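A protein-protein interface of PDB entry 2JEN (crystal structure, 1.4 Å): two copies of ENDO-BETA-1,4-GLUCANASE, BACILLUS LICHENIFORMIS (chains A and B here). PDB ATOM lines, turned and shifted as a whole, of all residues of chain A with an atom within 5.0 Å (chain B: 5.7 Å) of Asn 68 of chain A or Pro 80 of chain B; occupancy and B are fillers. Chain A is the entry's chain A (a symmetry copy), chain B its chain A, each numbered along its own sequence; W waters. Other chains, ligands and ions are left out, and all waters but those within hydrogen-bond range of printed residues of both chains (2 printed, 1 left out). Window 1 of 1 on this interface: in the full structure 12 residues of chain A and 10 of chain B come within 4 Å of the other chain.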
ATOM      1  N   ALA A  29     -24.503   9.199  24.268  1.00  0.00           N
ATOM      2  CA  ALA A  29     -24.151   7.759  24.429  1.00  0.00           C
ATOM      3  C   ALA A  29     -23.845   7.184  23.072  1.00  0.00           C
ATOM      4  O   ALA A  29     -24.368   7.635  22.064  1.00  0.00           O
ATOM      5  CB  ALA A  29     -25.314   7.014  25.079  1.00  0.00           C
ATOM      6  N   TYR A  66     -19.373   0.197  24.890  1.00  0.00           N
ATOM      7  CA  TYR A  66     -20.352   1.273  25.044  1.00  0.00           C
ATOM      8  C   TYR A  66     -19.945   2.285  26.082  1.00  0.00           C
ATOM      9  O   TYR A  66     -19.236   1.999  27.042  1.00  0.00           O
ATOM     10  CB  TYR A  66     -21.734   0.705  25.391  1.00  0.00           C
ATOM     11  CG  TYR A  66     -21.891   0.176  26.814  1.00  0.00           C
ATOM     12  CD1 TYR A  66     -21.594  -1.131  27.153  1.00  0.00           C
ATOM     13  CD2 TYR A  66     -22.359   1.001  27.801  1.00  0.00           C
ATOM     14  CE1 TYR A  66     -21.768  -1.584  28.436  1.00  0.00           C
ATOM     15  CE2 TYR A  66     -22.536   0.564  29.101  1.00  0.00           C
ATOM     16  CZ  TYR A  66     -22.218  -0.735  29.408  1.00  0.00           C
ATOM     17  OH  TYR A  66     -22.478  -1.205  30.698  1.00  0.00           O
ATOM     18  N   HIS A  67     -20.439   3.504  25.858  1.00  0.00           N
ATOM     19  CA  HIS A  67     -20.256   4.613  26.788  1.00  0.00           C
ATOM     20  C   HIS A  67     -21.549   5.356  26.894  1.00  0.00           C
ATOM     21  O   HIS A  67     -21.982   5.950  25.906  1.00  0.00           O
ATOM     22  CB  HIS A  67     -19.149   5.547  26.267  1.00  0.00           C
ATOM     23  CG  HIS A  67     -18.867   6.741  27.130  1.00  0.00           C
ATOM     24  ND1 HIS A  67     -19.551   7.928  26.983  1.00  0.00           N
ATOM     25  CD2 HIS A  67     -17.974   6.935  28.127  1.00  0.00           C
ATOM     26  CE1 HIS A  67     -19.101   8.794  27.876  1.00  0.00           C
ATOM     27  NE2 HIS A  67     -18.130   8.225  28.577  1.00  0.00           N
ATOM     28  N   ASN A  68     -22.181   5.318  28.064  1.00  0.00           N
ATOM     29  CA  ASN A  68     -23.358   6.150  28.342  1.00  0.00           C
ATOM     30  C   ASN A  68     -22.944   7.461  29.022  1.00  0.00           C
ATOM     31  O   ASN A  68     -23.443   8.520  28.685  1.00  0.00           O
ATOM     32  CB  ASN A  68     -24.372   5.399  29.195  1.00  0.00           C
ATOM     33  CG  ASN A  68     -24.875   4.135  28.551  1.00  0.00           C
ATOM     34  OD1 ASN A  68     -24.993   4.060  27.310  1.00  0.00           O
ATOM     35  ND2 ASN A  68     -25.167   3.129  29.372  1.00  0.00           N
ATOM     36  N   SER A  69     -22.052   7.354  29.988  1.00  0.00           N
ATOM     37  CA  SER A  69     -21.407   8.491  30.630  1.00  0.00           C
ATOM     38  C   SER A  69     -20.040   8.027  31.133  1.00  0.00           C
ATOM     39  O   SER A  69     -19.740   6.824  31.138  1.00  0.00           O
ATOM     40  CB  SER A  69     -22.220   8.973  31.821  1.00  0.00           C
ATOM     41  OG  SER A  69     -22.084   8.089  32.902  1.00  0.00           O
ATOM     42  N   ASP A  70     -19.288   8.953  31.725  1.00  0.00           N
ATOM     43  CA  ASP A  70     -18.009   8.586  32.281  1.00  0.00           C
ATOM     44  C   ASP A  70     -18.108   7.722  33.548  1.00  0.00           C
ATOM     45  O   ASP A  70     -17.076   7.232  34.055  1.00  0.00           O
ATOM     46  CB  ASP A  70     -17.173   9.821  32.574  1.00  0.00           C
ATOM     47  CG  ASP A  70     -16.819  10.640  31.355  1.00  0.00           C
ATOM     48  OD1 ASP A  70     -17.024  10.230  30.199  1.00  0.00           O
ATOM     49  OD2 ASP A  70     -16.303  11.771  31.590  1.00  0.00           O
ATOM     50  N   ASP A  72     -20.697   5.251  33.539  1.00  0.00           N
ATOM     51  CA  ASP A  72     -21.606   4.201  33.086  1.00  0.00           C
ATOM     52  C   ASP A  72     -21.170   3.795  31.689  1.00  0.00           C
ATOM     53  O   ASP A  72     -21.646   4.307  30.677  1.00  0.00           O
ATOM     54  CB  ASP A  72     -23.056   4.717  33.104  1.00  0.00           C
ATOM     55  CG  ASP A  72     -24.070   3.632  32.807  1.00  0.00           C
ATOM     56  OD1 ASP A  72     -23.821   2.443  33.170  1.00  0.00           O
ATOM     57  OD2 ASP A  72     -25.170   3.974  32.263  1.00  0.00           O
ATOM     58  N   MET A  73     -20.300   2.812  31.638  1.00  0.00           N
ATOM     59  CA  MET A  73     -19.648   2.396  30.399  1.00  0.00           C
ATOM     60  C   MET A  73     -19.217   0.963  30.546  1.00  0.00           C
ATOM     61  O   MET A  73     -19.190   0.446  31.689  1.00  0.00           O
ATOM     62  CB  MET A  73     -18.472   3.307  30.071  1.00  0.00           C
ATOM     63  CG  MET A  73     -17.378   3.281  31.088  1.00  0.00           C
ATOM     64  SD  MET A  73     -16.051   4.456  30.726  1.00  0.00           S
ATOM     65  CE  MET A  73     -15.300   4.671  32.349  1.00  0.00           C
ATOM     66  N   VAL A  76     -19.744  -5.809  26.186  1.00  0.00           N
ATOM     67  CA  VAL A  76     -20.544  -6.988  26.146  1.00  0.00           C
ATOM     68  C   VAL A  76     -19.853  -7.921  25.137  1.00  0.00           C
ATOM     69  O   VAL A  76     -19.384  -7.451  24.101  1.00  0.00           O
ATOM     70  CB  VAL A  76     -21.945  -6.561  25.681  1.00  0.00           C
ATOM     71  CG1 VAL A  76     -22.923  -7.714  25.845  1.00  0.00           C
ATOM     72  CG2 VAL A  76     -22.400  -5.256  26.454  1.00  0.00           C
ATOM     73  N   GLN A 250     -20.728  -9.556  30.244  1.00  0.00           N
ATOM     74  CA  GLN A 250     -20.520  -8.152  30.150  1.00  0.00           C
ATOM     75  C   GLN A 250     -19.860  -7.623  31.401  1.00  0.00           C
ATOM     76  O   GLN A 250     -19.931  -8.254  32.480  1.00  0.00           O
ATOM     77  CB  GLN A 250     -21.847  -7.447  29.935  1.00  0.00           C
ATOM     78  CG  GLN A 250     -22.776  -7.465  31.124  1.00  0.00           C
ATOM     79  CD  GLN A 250     -24.139  -6.935  30.785  1.00  0.00           C
ATOM     80  OE1 GLN A 250     -24.315  -5.722  30.536  1.00  0.00           O
ATOM     81  NE2 GLN A 250     -25.124  -7.834  30.763  1.00  0.00           N
ATOM     82  N   ASN A 252     -19.658  -3.702  33.469  1.00  0.00           N
ATOM     83  CA  ASN A 252     -20.030  -2.317  33.575  1.00  0.00           C
ATOM     84  C   ASN A 252     -19.077  -1.672  34.550  1.00  0.00           C
ATOM     85  O   ASN A 252     -18.754  -2.262  35.601  1.00  0.00           O
ATOM     86  CB  ASN A 252     -21.470  -2.167  34.072  1.00  0.00           C
ATOM     87  CG  ASN A 252     -21.837  -0.744  34.292  1.00  0.00           C
ATOM     88  OD1 ASN A 252     -22.347  -0.013  33.354  1.00  0.00           O
ATOM     89  ND2 ASN A 252     -21.579  -0.293  35.474  1.00  0.00           N
ATOM     90  N   GLN B  57     -30.813   8.318  26.540  1.00  0.00           N
ATOM     91  CA  GLN B  57     -29.455   8.678  26.891  1.00  0.00           C
ATOM     92  C   GLN B  57     -28.521   7.500  27.119  1.00  0.00           C
ATOM     93  O   GLN B  57     -27.426   7.664  27.668  1.00  0.00           O
ATOM     94  CB  GLN B  57     -29.451   9.597  28.126  1.00  0.00           C
ATOM     95  CG  GLN B  57     -30.234  10.890  27.935  1.00  0.00           C
ATOM     96  CD  GLN B  57     -30.115  11.782  29.123  1.00  0.00           C
ATOM     97  OE1 GLN B  57     -30.900  11.690  30.049  1.00  0.00           O
ATOM     98  NE2 GLN B  57     -29.114  12.642  29.111  1.00  0.00           N
ATOM     99  N   VAL B  58     -28.935   6.325  26.658  1.00  0.00           N
ATOM    100  CA  VAL B  58     -28.109   5.114  26.748  1.00  0.00           C
ATOM    101  C   VAL B  58     -27.960   4.440  25.396  1.00  0.00           C
ATOM    102  O   VAL B  58     -28.743   4.697  24.478  1.00  0.00           O
ATOM    103  CB  VAL B  58     -28.594   4.135  27.836  1.00  0.00           C
ATOM    104  CG1 VAL B  58     -28.554   4.812  29.249  1.00  0.00           C
ATOM    105  CG2 VAL B  58     -29.994   3.613  27.547  1.00  0.00           C
ATOM    106  N   SER B  59     -26.990   3.550  25.299  1.00  0.00           N
ATOM    107  CA  SER B  59     -26.687   2.882  24.048  1.00  0.00           C
ATOM    108  C   SER B  59     -26.270   1.438  24.331  1.00  0.00           C
ATOM    109  O   SER B  59     -26.136   1.041  25.479  1.00  0.00           O
ATOM    110  CB  SER B  59     -25.600   3.641  23.276  1.00  0.00           C
ATOM    111  OG  SER B  59     -25.400   3.117  21.971  1.00  0.00           O
ATOM    112  N   GLY B  60     -26.087   0.666  23.288  1.00  0.00           N
ATOM    113  CA  GLY B  60     -25.687  -0.706  23.432  1.00  0.00           C
ATOM    114  C   GLY B  60     -26.792  -1.697  23.675  1.00  0.00           C
ATOM    115  O   GLY B  60     -26.520  -2.841  24.034  1.00  0.00           O
ATOM    116  N   TRP B  61     -28.029  -1.250  23.550  1.00  0.00           N
ATOM    117  CA  TRP B  61     -29.170  -2.013  23.997  1.00  0.00           C
ATOM    118  C   TRP B  61     -29.970  -2.624  22.869  1.00  0.00           C
ATOM    119  O   TRP B  61     -29.877  -2.215  21.704  1.00  0.00           O
ATOM    120  CB  TRP B  61     -30.088  -1.110  24.832  1.00  0.00           C
ATOM    121  CG  TRP B  61     -30.659   0.064  24.131  1.00  0.00           C
ATOM    122  CD1 TRP B  61     -30.199   1.370  24.158  1.00  0.00           C
ATOM    123  CD2 TRP B  61     -31.890   0.093  23.388  1.00  0.00           C
ATOM    124  NE1 TRP B  61     -31.065   2.182  23.465  1.00  0.00           N
ATOM    125  CE2 TRP B  61     -32.108   1.430  22.983  1.00  0.00           C
ATOM    126  CE3 TRP B  61     -32.853  -0.862  23.091  1.00  0.00           C
ATOM    127  CZ2 TRP B  61     -33.257   1.796  22.299  1.00  0.00           C
ATOM    128  CZ3 TRP B  61     -33.983  -0.480  22.413  1.00  0.00           C
ATOM    129  CH2 TRP B  61     -34.164   0.847  22.030  1.00  0.00           C
ATOM    130  N   ASN B  78     -31.551  -6.440  26.564  1.00  0.00           N
ATOM    131  CA  ASN B  78     -30.214  -6.138  26.997  1.00  0.00           C
ATOM    132  C   ASN B  78     -30.051  -4.646  27.175  1.00  0.00           C
ATOM    133  O   ASN B  78     -30.177  -3.899  26.205  1.00  0.00           O
ATOM    134  CB  ASN B  78     -29.210  -6.599  25.931  1.00  0.00           C
ATOM    135  CG  ASN B  78     -27.802  -6.240  26.251  1.00  0.00           C
ATOM    136  OD1 ASN B  78     -27.360  -6.374  27.377  1.00  0.00           O
ATOM    137  ND2 ASN B  78     -27.088  -5.737  25.268  1.00  0.00           N
ATOM    138  N   TRP B  79     -29.858  -4.215  28.433  1.00  0.00           N
ATOM    139  CA  TRP B  79     -29.864  -2.804  28.852  1.00  0.00           C
ATOM    140  C   TRP B  79     -28.550  -2.567  29.647  1.00  0.00           C
ATOM    141  O   TRP B  79     -28.539  -2.562  30.880  1.00  0.00           O
ATOM    142  CB  TRP B  79     -31.088  -2.442  29.687  1.00  0.00           C
ATOM    143  CG  TRP B  79     -32.288  -2.353  28.832  1.00  0.00           C
ATOM    144  CD1 TRP B  79     -33.277  -3.264  28.713  1.00  0.00           C
ATOM    145  CD2 TRP B  79     -32.599  -1.304  27.914  1.00  0.00           C
ATOM    146  NE1 TRP B  79     -34.210  -2.852  27.778  1.00  0.00           N
ATOM    147  CE2 TRP B  79     -33.782  -1.661  27.253  1.00  0.00           C
ATOM    148  CE3 TRP B  79     -31.986  -0.107  27.581  1.00  0.00           C
ATOM    149  CZ2 TRP B  79     -34.368  -0.840  26.309  1.00  0.00           C
ATOM    150  CZ3 TRP B  79     -32.578   0.716  26.655  1.00  0.00           C
ATOM    151  CH2 TRP B  79     -33.751   0.332  26.013  1.00  0.00           C
ATOM    152  N   PRO B  80     -27.406  -2.420  28.956  1.00  0.00           N
ATOM    153  CA  PRO B  80     -26.168  -2.255  29.718  1.00  0.00           C
ATOM    154  C   PRO B  80     -26.018  -0.886  30.380  1.00  0.00           C
ATOM    155  O   PRO B  80     -25.613   0.085  29.755  1.00  0.00           O
ATOM    156  CB  PRO B  80     -25.062  -2.524  28.685  1.00  0.00           C
ATOM    157  CG  PRO B  80     -25.735  -3.132  27.525  1.00  0.00           C
ATOM    158  CD  PRO B  80     -27.116  -2.553  27.524  1.00  0.00           C
ATOM    159  N   SER B  81     -26.334  -0.822  31.666  1.00  0.00           N
ATOM    160  CA  SER B  81     -26.268   0.417  32.439  1.00  0.00           C
ATOM    161  C   SER B  81     -26.342   0.101  33.938  1.00  0.00           C
ATOM    162  O   SER B  81     -27.047  -0.822  34.344  1.00  0.00           O
ATOM    163  CB  SER B  81     -27.476   1.294  32.109  1.00  0.00           C
ATOM    164  OG  SER B  81     -27.449   2.531  32.874  1.00  0.00           O
ATOM    165  N   ASN B  82     -25.653   0.913  34.726  1.00  0.00           N
ATOM    166  CA  ASN B  82     -25.677   0.807  36.181  1.00  0.00           C
ATOM    167  C   ASN B  82     -26.621   1.786  36.863  1.00  0.00           C
ATOM    168  O   ASN B  82     -26.736   1.752  38.098  1.00  0.00           O
ATOM    169  CB  ASN B  82     -24.275   0.949  36.769  1.00  0.00           C
ATOM    170  CG  ASN B  82     -23.668   2.313  36.523  1.00  0.00           C
ATOM    171  OD1 ASN B  82     -24.354   3.343  36.675  1.00  0.00           O
ATOM    172  ND2 ASN B  82     -22.382   2.358  36.164  1.00  0.00           N
ATOM    173  N   GLY B 246     -31.126  -2.098  34.398  1.00  0.00           N
ATOM    174  CA  GLY B 246     -29.927  -2.561  33.710  1.00  0.00           C
ATOM    175  C   GLY B 246     -29.862  -4.059  33.691  1.00  0.00           C
ATOM    176  O   GLY B 246     -30.500  -4.718  34.524  1.00  0.00           O
ATOM    177  N   GLY B 247     -29.081  -4.608  32.777  1.00  0.00           N
ATOM    178  CA  GLY B 247     -28.889  -6.042  32.678  1.00  0.00           C
ATOM    179  C   GLY B 247     -29.546  -6.660  31.460  1.00  0.00           C
ATOM    180  O   GLY B 247     -30.157  -5.965  30.628  1.00  0.00           O
HETATM  181  O   HOH W   1     -25.396   9.956  26.827  1.00  0.00           O
HETATM  182  O   HOH W   2     -26.505   8.372  30.211  1.00  0.00           O
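No position is printed for both chains.
Of the 12 pairs that touch across the chains among the printed residues, none has its exchanged pair printed and touching as well.
Hydrophobic or aromatic side chains of chain B that line the printed part of chain A: Val 58 and Pro 80.
Of the 11 printed residues of chain A, 6 touch a printed residue of chain B.
Hydrophobic or aromatic side chains of chain A within 4 Å of the printed part of chain B: Ala 29 and Tyr 66.
Among the printed residues, 12 pairs touch across the chains.
Among the printed residues, no Asp or Glu carboxylate lies within 4 Å of a Lys or Arg side-chain nitrogen of the other chain.
The backbone NH of Ser 59 of chain B lies within hydrogen-bond range of the side-chain amide oxygen of Asn 68 of chain A (2.9 Å).
The backbone carbonyl oxygen (O) of Pro 80 of chain B is in hydrogen-bond range of the side-chain amide nitrogen (ND2) of Asn 68 of chain A, 3.1 Å away.
The side-chain hydroxyl (OG) of Ser 81 of chain B is in hydrogen-bond range of the side-chain carboxylate (OD2) of Asp 72 of chain A, 2.8 Å away.
The backbone NH of Asn 82 of chain B is in hydrogen-bond range of the side-chain carboxylate of Asp 72 of chain A, 2.8 Å away.
The side-chain amide nitrogen (ND2) of Asn 82 of chain B lies close to the side-chain amide nitrogen (ND2) of Asn 252 of chain A, at 2.9 Å.
Among the printed residues, merely in contact across the chains: Ala 29 of chain A with Gln 57 of chain B (3.4 Å), Ala 29 of chain A with Val 58 of chain B (3.7 Å), Ala 29 of chain A with Ser 59 of chain B (3.8 Å), Tyr 66 of chain A with Pro 80 of chain B (3.2 Å), Tyr 66 of chain A with Ser 81 of chain B (3.99 Å), Asn 68 of chain A with Val 58 of chain B (3.3 Å) and Gln 250 of chain A with Pro 80 of chain B (3.8 Å).
Water W2 lies within hydrogen-bond range of the backbone carbonyl oxygen of Gln 57 of chain B (2.8 Å) and the backbone carbonyl oxygen of Asn 68 of chain A (3.4 Å).
Water W1 lies within hydrogen-bond range of N of Ala 29 of chain A, O of Asn 68 of chain A and O of Gln 57 of chain B.
Printed residues of chain A within 4 Å of Pro 80 of chain B: Tyr 66 (3.2 Å), Asn 68 (3.1 Å) and Gln 250 (3.8 Å).
Of the printed residues of chain B, Ala 29 of chain A touches Gln 57, Val 58 and Ser 59.
Of the printed residues of chain B, Asp 72 of chain A touches Ser 81 and Asn 82.
Printed residues of chain A within 4 Å of Asn 82 of chain B: Asp 72 (2.8 Å) and Asn 252 (2.9 Å).
His 67 of chain A touches none of the printed residues of chain B.
The nearest printed residue of chain B that does not touch Asn 68 of chain A is Ser 81 of chain B (4.02 Å).
The nearest printed residue of chain A that does not touch Ser 59 of chain B is Tyr 66 of chain A (4.4 Å).
OH of Tyr 66 of chain A lies within hydrogen-bond range of OD1 of Asn 252 of chain A (2.9 Å).
The side-chain amide nitrogen (ND2) of Asn 68 of chain A is in hydrogen-bond range of the side-chain carboxylate (OD2) of Asp 72 of chain A (3.0 Å).
The side-chain hydroxyl of Ser 69 of chain A is in hydrogen-bond range of the backbone NH of Asp 72 of chain A (3.2 Å).
The side-chain carboxylate of Asp 72 of chain A sits close to the side-chain amide oxygen of Asn 252 of chain A (2.9 Å).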
